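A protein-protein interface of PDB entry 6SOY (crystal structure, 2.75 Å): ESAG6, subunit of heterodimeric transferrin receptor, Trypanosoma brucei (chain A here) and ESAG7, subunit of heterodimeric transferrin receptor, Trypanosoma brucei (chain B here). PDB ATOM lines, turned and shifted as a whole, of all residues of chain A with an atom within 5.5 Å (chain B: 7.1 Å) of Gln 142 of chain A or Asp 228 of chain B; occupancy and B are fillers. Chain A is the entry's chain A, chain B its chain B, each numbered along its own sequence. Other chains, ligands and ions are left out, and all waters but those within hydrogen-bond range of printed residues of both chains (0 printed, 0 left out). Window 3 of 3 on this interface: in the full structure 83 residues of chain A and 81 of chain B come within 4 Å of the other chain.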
ATOM      1  N   ALA A 136     -20.775   6.760 -12.892  1.00  0.00           N
ATOM      2  CA  ALA A 136     -21.281   5.502 -12.359  1.00  0.00           C
ATOM      3  C   ALA A 136     -21.163   4.422 -13.392  1.00  0.00           C
ATOM      4  O   ALA A 136     -22.183   3.898 -13.813  1.00  0.00           O
ATOM      5  CB  ALA A 136     -22.734   5.669 -11.939  1.00  0.00           C
ATOM      6  N   ALA A 137     -19.936   4.078 -13.828  1.00  0.00           N
ATOM      7  CA  ALA A 137     -19.741   3.064 -14.886  1.00  0.00           C
ATOM      8  C   ALA A 137     -18.522   2.169 -14.637  1.00  0.00           C
ATOM      9  O   ALA A 137     -17.466   2.656 -14.235  1.00  0.00           O
ATOM     10  CB  ALA A 137     -19.631   3.750 -16.232  1.00  0.00           C
ATOM     11  N   GLY A 138     -18.689   0.873 -14.831  1.00  0.00           N
ATOM     12  CA  GLY A 138     -17.624  -0.101 -14.626  1.00  0.00           C
ATOM     13  C   GLY A 138     -17.499  -1.130 -15.735  1.00  0.00           C
ATOM     14  O   GLY A 138     -18.056  -0.954 -16.826  1.00  0.00           O
ATOM     15  N   ARG A 139     -16.746  -2.218 -15.459  1.00  0.00           N
ATOM     16  CA  ARG A 139     -16.511  -3.358 -16.372  1.00  0.00           C
ATOM     17  C   ARG A 139     -17.777  -4.227 -16.540  1.00  0.00           C
ATOM     18  O   ARG A 139     -18.852  -3.843 -16.062  1.00  0.00           O
ATOM     19  CB  ARG A 139     -15.337  -4.215 -15.842  1.00  0.00           C
ATOM     20  CG  ARG A 139     -13.968  -3.631 -16.185  1.00  0.00           C
ATOM     21  CD  ARG A 139     -12.837  -4.319 -15.446  1.00  0.00           C
ATOM     22  NE  ARG A 139     -11.537  -3.762 -15.826  1.00  0.00           N
ATOM     23  CZ  ARG A 139     -10.745  -4.269 -16.767  1.00  0.00           C
ATOM     24  NH1 ARG A 139      -9.582  -3.697 -17.044  1.00  0.00           N
ATOM     25  NH2 ARG A 139     -11.109  -5.359 -17.436  1.00  0.00           N
ATOM     26  N   SER A 140     -17.655  -5.395 -17.214  1.00  0.00           N
ATOM     27  CA  SER A 140     -18.745  -6.369 -17.432  1.00  0.00           C
ATOM     28  C   SER A 140     -20.105  -5.737 -17.885  1.00  0.00           C
ATOM     29  O   SER A 140     -21.166  -6.216 -17.471  1.00  0.00           O
ATOM     30  CB  SER A 140     -18.935  -7.250 -16.190  1.00  0.00           C
ATOM     31  OG  SER A 140     -18.162  -8.444 -16.202  1.00  0.00           O
ATOM     32  N   SER A 141     -20.059  -4.670 -18.737  1.00  0.00           N
ATOM     33  CA  SER A 141     -21.233  -3.961 -19.262  1.00  0.00           C
ATOM     34  C   SER A 141     -22.226  -3.609 -18.144  1.00  0.00           C
ATOM     35  O   SER A 141     -23.385  -4.030 -18.150  1.00  0.00           O
ATOM     36  CB  SER A 141     -21.901  -4.764 -20.382  1.00  0.00           C
ATOM     37  OG  SER A 141     -21.487  -4.371 -21.685  1.00  0.00           O
ATOM     38  N   GLN A 142     -21.713  -2.890 -17.145  1.00  0.00           N
ATOM     39  CA  GLN A 142     -22.392  -2.390 -15.952  1.00  0.00           C
ATOM     40  C   GLN A 142     -22.203  -0.874 -16.017  1.00  0.00           C
ATOM     41  O   GLN A 142     -21.068  -0.398 -16.106  1.00  0.00           O
ATOM     42  CB  GLN A 142     -21.721  -2.990 -14.723  1.00  0.00           C
ATOM     43  CG  GLN A 142     -22.692  -3.529 -13.684  1.00  0.00           C
ATOM     44  CD  GLN A 142     -23.301  -4.879 -13.971  1.00  0.00           C
ATOM     45  OE1 GLN A 142     -23.246  -5.420 -15.089  1.00  0.00           O
ATOM     46  NE2 GLN A 142     -23.919  -5.450 -12.952  1.00  0.00           N
ATOM     47  N   PHE A 143     -23.303  -0.116 -16.099  1.00  0.00           N
ATOM     48  CA  PHE A 143     -23.248   1.331 -16.323  1.00  0.00           C
ATOM     49  C   PHE A 143     -24.581   1.996 -15.996  1.00  0.00           C
ATOM     50  O   PHE A 143     -25.578   1.288 -15.878  1.00  0.00           O
ATOM     51  CB  PHE A 143     -22.939   1.568 -17.813  1.00  0.00           C
ATOM     52  CG  PHE A 143     -23.744   0.706 -18.763  1.00  0.00           C
ATOM     53  CD1 PHE A 143     -25.034   1.062 -19.127  1.00  0.00           C
ATOM     54  CD2 PHE A 143     -23.219  -0.468 -19.275  1.00  0.00           C
ATOM     55  CE1 PHE A 143     -25.782   0.250 -19.966  1.00  0.00           C
ATOM     56  CE2 PHE A 143     -23.979  -1.288 -20.107  1.00  0.00           C
ATOM     57  CZ  PHE A 143     -25.242  -0.914 -20.462  1.00  0.00           C
ATOM     58  N   CYS A 144     -24.629   3.354 -15.954  1.00  0.00           N
ATOM     59  CA  CYS A 144     -25.873   4.105 -15.673  1.00  0.00           C
ATOM     60  C   CYS A 144     -26.349   4.974 -16.870  1.00  0.00           C
ATOM     61  O   CYS A 144     -27.478   5.472 -16.854  1.00  0.00           O
ATOM     62  CB  CYS A 144     -25.764   4.908 -14.375  1.00  0.00           C
ATOM     63  SG  CYS A 144     -25.842   3.882 -12.873  1.00  0.00           S
ATOM     64  N   PRO A 152     -20.627   1.080 -21.107  1.00  0.00           N
ATOM     65  CA  PRO A 152     -20.964   2.467 -20.705  1.00  0.00           C
ATOM     66  C   PRO A 152     -20.807   3.463 -21.841  1.00  0.00           C
ATOM     67  O   PRO A 152     -20.043   3.221 -22.783  1.00  0.00           O
ATOM     68  CB  PRO A 152     -19.912   2.789 -19.634  1.00  0.00           C
ATOM     69  CG  PRO A 152     -19.363   1.454 -19.192  1.00  0.00           C
ATOM     70  CD  PRO A 152     -19.420   0.598 -20.414  1.00  0.00           C
ATOM     71  N   LYS A 212     -29.362  -6.085 -17.784  1.00  0.00           N
ATOM     72  CA  LYS A 212     -28.464  -6.492 -16.699  1.00  0.00           C
ATOM     73  C   LYS A 212     -27.245  -5.559 -16.509  1.00  0.00           C
ATOM     74  O   LYS A 212     -26.100  -6.019 -16.345  1.00  0.00           O
ATOM     75  CB  LYS A 212     -28.032  -7.973 -16.878  1.00  0.00           C
ATOM     76  CG  LYS A 212     -27.523  -8.332 -18.278  1.00  0.00           C
ATOM     77  CD  LYS A 212     -27.100  -9.790 -18.397  1.00  0.00           C
ATOM     78  CE  LYS A 212     -28.240 -10.718 -18.768  1.00  0.00           C
ATOM     79  NZ  LYS A 212     -27.863 -12.157 -18.638  1.00  0.00           N
ATOM     80  N   ASP A 213     -27.505  -4.248 -16.489  1.00  0.00           N
ATOM     81  CA  ASP A 213     -26.427  -3.287 -16.360  1.00  0.00           C
ATOM     82  C   ASP A 213     -26.190  -2.792 -14.936  1.00  0.00           C
ATOM     83  O   ASP A 213     -25.420  -1.844 -14.760  1.00  0.00           O
ATOM     84  CB  ASP A 213     -26.604  -2.116 -17.334  1.00  0.00           C
ATOM     85  CG  ASP A 213     -27.896  -1.336 -17.239  1.00  0.00           C
ATOM     86  OD1 ASP A 213     -28.182  -0.775 -16.152  1.00  0.00           O
ATOM     87  OD2 ASP A 213     -28.597  -1.248 -18.255  1.00  0.00           O
ATOM     88  N   GLY A 214     -26.823  -3.441 -13.953  1.00  0.00           N
ATOM     89  CA  GLY A 214     -26.677  -3.149 -12.528  1.00  0.00           C
ATOM     90  C   GLY A 214     -26.662  -1.695 -12.093  1.00  0.00           C
ATOM     91  O   GLY A 214     -25.880  -1.323 -11.216  1.00  0.00           O
ATOM     92  N   ALA B 221     -17.382   0.664  -4.677  1.00  0.00           N
ATOM     93  CA  ALA B 221     -17.235  -0.799  -4.742  1.00  0.00           C
ATOM     94  C   ALA B 221     -18.523  -1.442  -5.207  1.00  0.00           C
ATOM     95  O   ALA B 221     -19.564  -0.779  -5.270  1.00  0.00           O
ATOM     96  CB  ALA B 221     -16.854  -1.370  -3.383  1.00  0.00           C
ATOM     97  N   ASP B 222     -18.457  -2.740  -5.521  1.00  0.00           N
ATOM     98  CA  ASP B 222     -19.606  -3.534  -5.945  1.00  0.00           C
ATOM     99  C   ASP B 222     -20.713  -3.390  -4.863  1.00  0.00           C
ATOM    100  O   ASP B 222     -20.395  -3.233  -3.686  1.00  0.00           O
ATOM    101  CB  ASP B 222     -19.174  -4.987  -6.143  1.00  0.00           C
ATOM    102  CG  ASP B 222     -19.057  -5.745  -4.846  1.00  0.00           C
ATOM    103  OD1 ASP B 222     -18.040  -5.556  -4.136  1.00  0.00           O
ATOM    104  OD2 ASP B 222     -20.006  -6.486  -4.510  1.00  0.00           O
ATOM    105  N   GLY B 223     -21.972  -3.322  -5.292  1.00  0.00           N
ATOM    106  CA  GLY B 223     -23.121  -3.126  -4.410  1.00  0.00           C
ATOM    107  C   GLY B 223     -23.335  -1.686  -3.995  1.00  0.00           C
ATOM    108  O   GLY B 223     -24.126  -1.426  -3.090  1.00  0.00           O
ATOM    109  N   GLY B 224     -22.615  -0.757  -4.638  1.00  0.00           N
ATOM    110  CA  GLY B 224     -22.717   0.680  -4.388  1.00  0.00           C
ATOM    111  C   GLY B 224     -23.463   1.398  -5.496  1.00  0.00           C
ATOM    112  O   GLY B 224     -24.669   1.187  -5.669  1.00  0.00           O
ATOM    113  N   LEU B 225     -22.747   2.231  -6.280  1.00  0.00           N
ATOM    114  CA  LEU B 225     -23.324   2.938  -7.434  1.00  0.00           C
ATOM    115  C   LEU B 225     -23.810   1.898  -8.454  1.00  0.00           C
ATOM    116  O   LEU B 225     -24.936   2.000  -8.945  1.00  0.00           O
ATOM    117  CB  LEU B 225     -22.318   3.950  -8.044  1.00  0.00           C
ATOM    118  CG  LEU B 225     -21.867   5.082  -7.069  1.00  0.00           C
ATOM    119  CD1 LEU B 225     -20.484   5.571  -7.381  1.00  0.00           C
ATOM    120  CD2 LEU B 225     -22.871   6.229  -7.006  1.00  0.00           C
ATOM    121  N   LEU B 226     -22.992   0.837  -8.661  1.00  0.00           N
ATOM    122  CA  LEU B 226     -23.241  -0.323  -9.509  1.00  0.00           C
ATOM    123  C   LEU B 226     -23.429  -1.528  -8.582  1.00  0.00           C
ATOM    124  O   LEU B 226     -22.720  -1.638  -7.582  1.00  0.00           O
ATOM    125  CB  LEU B 226     -22.024  -0.531 -10.414  1.00  0.00           C
ATOM    126  CG  LEU B 226     -21.997   0.057 -11.837  1.00  0.00           C
ATOM    127  CD1 LEU B 226     -23.042   1.166 -12.083  1.00  0.00           C
ATOM    128  CD2 LEU B 226     -20.616   0.498 -12.182  1.00  0.00           C
ATOM    129  N   LYS B 227     -24.353  -2.441  -8.909  1.00  0.00           N
ATOM    130  CA  LYS B 227     -24.693  -3.553  -8.008  1.00  0.00           C
ATOM    131  C   LYS B 227     -23.724  -4.755  -7.979  1.00  0.00           C
ATOM    132  O   LYS B 227     -23.689  -5.453  -6.977  1.00  0.00           O
ATOM    133  CB  LYS B 227     -26.141  -4.031  -8.256  1.00  0.00           C
ATOM    134  CG  LYS B 227     -26.357  -5.221  -9.169  1.00  0.00           C
ATOM    135  CD  LYS B 227     -27.533  -6.006  -8.635  1.00  0.00           C
ATOM    136  CE  LYS B 227     -27.564  -7.444  -9.068  1.00  0.00           C
ATOM    137  NZ  LYS B 227     -28.399  -8.248  -8.141  1.00  0.00           N
ATOM    138  N   ASP B 228     -22.968  -5.010  -9.030  1.00  0.00           N
ATOM    139  CA  ASP B 228     -22.099  -6.183  -9.050  1.00  0.00           C
ATOM    140  C   ASP B 228     -20.621  -5.882  -9.278  1.00  0.00           C
ATOM    141  O   ASP B 228     -19.815  -6.813  -9.219  1.00  0.00           O
ATOM    142  CB  ASP B 228     -22.582  -7.154 -10.156  1.00  0.00           C
ATOM    143  CG  ASP B 228     -23.981  -7.731  -9.973  1.00  0.00           C
ATOM    144  OD1 ASP B 228     -24.285  -8.221  -8.855  1.00  0.00           O
ATOM    145  OD2 ASP B 228     -24.762  -7.729 -10.961  1.00  0.00           O
ATOM    146  N   VAL B 229     -20.250  -4.612  -9.559  1.00  0.00           N
ATOM    147  CA  VAL B 229     -18.862  -4.332  -9.908  1.00  0.00           C
ATOM    148  C   VAL B 229     -18.289  -2.980  -9.339  1.00  0.00           C
ATOM    149  O   VAL B 229     -19.053  -2.077  -9.014  1.00  0.00           O
ATOM    150  CB  VAL B 229     -18.773  -4.442 -11.473  1.00  0.00           C
ATOM    151  CG1 VAL B 229     -19.177  -3.159 -12.180  1.00  0.00           C
ATOM    152  CG2 VAL B 229     -17.402  -4.914 -11.930  1.00  0.00           C
ATOM    153  N   CYS B 230     -16.928  -2.884  -9.211  1.00  0.00           N
ATOM    154  CA  CYS B 230     -16.166  -1.685  -8.835  1.00  0.00           C
ATOM    155  C   CYS B 230     -16.359  -0.756 -10.026  1.00  0.00           C
ATOM    156  O   CYS B 230     -16.578  -1.249 -11.133  1.00  0.00           O
ATOM    157  CB  CYS B 230     -14.670  -1.984  -8.675  1.00  0.00           C
ATOM    158  SG  CYS B 230     -14.232  -3.152  -7.358  1.00  0.00           S
ATOM    159  N   ASN B 232     -14.884   1.648 -13.061  1.00  0.00           N
ATOM    160  CA  ASN B 232     -13.727   1.607 -13.957  1.00  0.00           C
ATOM    161  C   ASN B 232     -12.835   2.856 -13.748  1.00  0.00           C
ATOM    162  O   ASN B 232     -11.851   3.033 -14.474  1.00  0.00           O
ATOM    163  CB  ASN B 232     -14.281   1.727 -15.384  1.00  0.00           C
ATOM    164  CG  ASN B 232     -14.152   0.525 -16.240  1.00  0.00           C
ATOM    165  OD1 ASN B 232     -13.165  -0.212 -16.200  1.00  0.00           O
ATOM    166  ND2 ASN B 232     -15.145   0.328 -17.070  1.00  0.00           N
ATOM    167  N   ARG B 233     -13.248   3.774 -12.842  1.00  0.00           N
ATOM    168  CA  ARG B 233     -12.703   5.124 -12.667  1.00  0.00           C
ATOM    169  C   ARG B 233     -12.957   5.716 -11.257  1.00  0.00           C
ATOM    170  O   ARG B 233     -13.690   5.133 -10.452  1.00  0.00           O
ATOM    171  CB  ARG B 233     -13.460   6.005 -13.687  1.00  0.00           C
ATOM    172  CG  ARG B 233     -14.938   5.539 -13.860  1.00  0.00           C
ATOM    173  CD  ARG B 233     -15.880   6.486 -14.568  1.00  0.00           C
ATOM    174  NE  ARG B 233     -15.705   6.557 -16.024  1.00  0.00           N
ATOM    175  CZ  ARG B 233     -16.010   5.588 -16.885  1.00  0.00           C
ATOM    176  NH1 ARG B 233     -16.426   4.407 -16.447  1.00  0.00           N
ATOM    177  NH2 ARG B 233     -15.841   5.773 -18.182  1.00  0.00           N
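The backbone carbonyl oxygen of Ala 137 of chain A sits at hydrogen-bond distance from the backbone NH of Asn 232 of chain B, 3.0 Å away.
O of Ala 137 of chain A lies within hydrogen-bond range of NH1 of Arg 233 of chain B.
The backbone carbonyl oxygen (O) of Gly 138 of chain A lies close to the side-chain amide nitrogen (ND2) of Asn 232 of chain B, at 3.2 Å.
The backbone NH (N) of Arg 139 of chain A sits close to the side-chain amide nitrogen (ND2) of Asn 232 of chain B (3.4 Å).
The side-chain carboxylate (OD2) of Asp 228 of chain B sits at hydrogen-bond distance from the side-chain amide nitrogen (NE2) of Gln 142 of chain A.
O of Gly 214 of chain A lies within hydrogen-bond range of N of Lys 227 of chain B (3.0 Å).
Hydrophobic or aromatic side chains of chain B within 4 Å of the printed part of chain A: Leu 226 and Val 229.
O of Ala 136 of chain A sits at hydrogen-bond distance from N of Cys 144 of chain A, at 3.3 Å.
The backbone carbonyl oxygen (O) of Ser 140 of chain A sits close to the side-chain amide oxygen (OE1) of Gln 142 of chain A, 3.3 Å away.
OE1 of Gln 142 of chain A sits close to O of Lys 212 of chain A, 3.2 Å away.
Of the printed residues of chain B, Ala 137 of chain A touches Leu 226 (3.6 Å), Asn 232 (3.0 Å) and Arg 233 (3.0 Å).
Of the printed residues of chain B, Gly 138 of chain A touches Leu 226, Cys 230 and Asn 232.
Ser 141 of chain A touches none of the printed residues of chain B.
Of the printed residues of chain B, Gln 142 of chain A touches Asp 228 and Val 229.
Asp 213 of chain A touches none of the printed residues of chain B.
Printed residues of chain B within 4 Å of Gly 214 of chain A: Leu 226 and Lys 227.
Of the printed residues of chain A, Leu 226 of chain B touches Ala 136 (3.3 Å), Ala 137 (3.6 Å), Gly 138 (3.3 Å), Cys 144 (3.98 Å) and Gly 214 (3.3 Å).
Asp 228 of chain B touches just one residue of chain A: Gln 142 (3.1 Å).
Of the printed residues of chain A, Arg 233 of chain B touches Ala 137 (3.0 Å).
Among the printed residues, merely in contact across the chains: Gly 138 of chain A with Leu 226 of chain B (3.3 Å), Gly 214 of chain A with Leu 226 of chain B (3.3 Å), Ala 136 of chain A with Leu 226 of chain B (3.3 Å), Gln 142 of chain A with Val 229 of chain B (3.6 Å), Ala 137 of chain A with Leu 226 of chain B (3.6 Å), Gly 138 of chain A with Cys 230 of chain B (3.8 Å), Arg 139 of chain A with Val 229 of chain B (3.96 Å) and Cys 144 of chain A with Leu 226 of chain B (3.98 Å).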
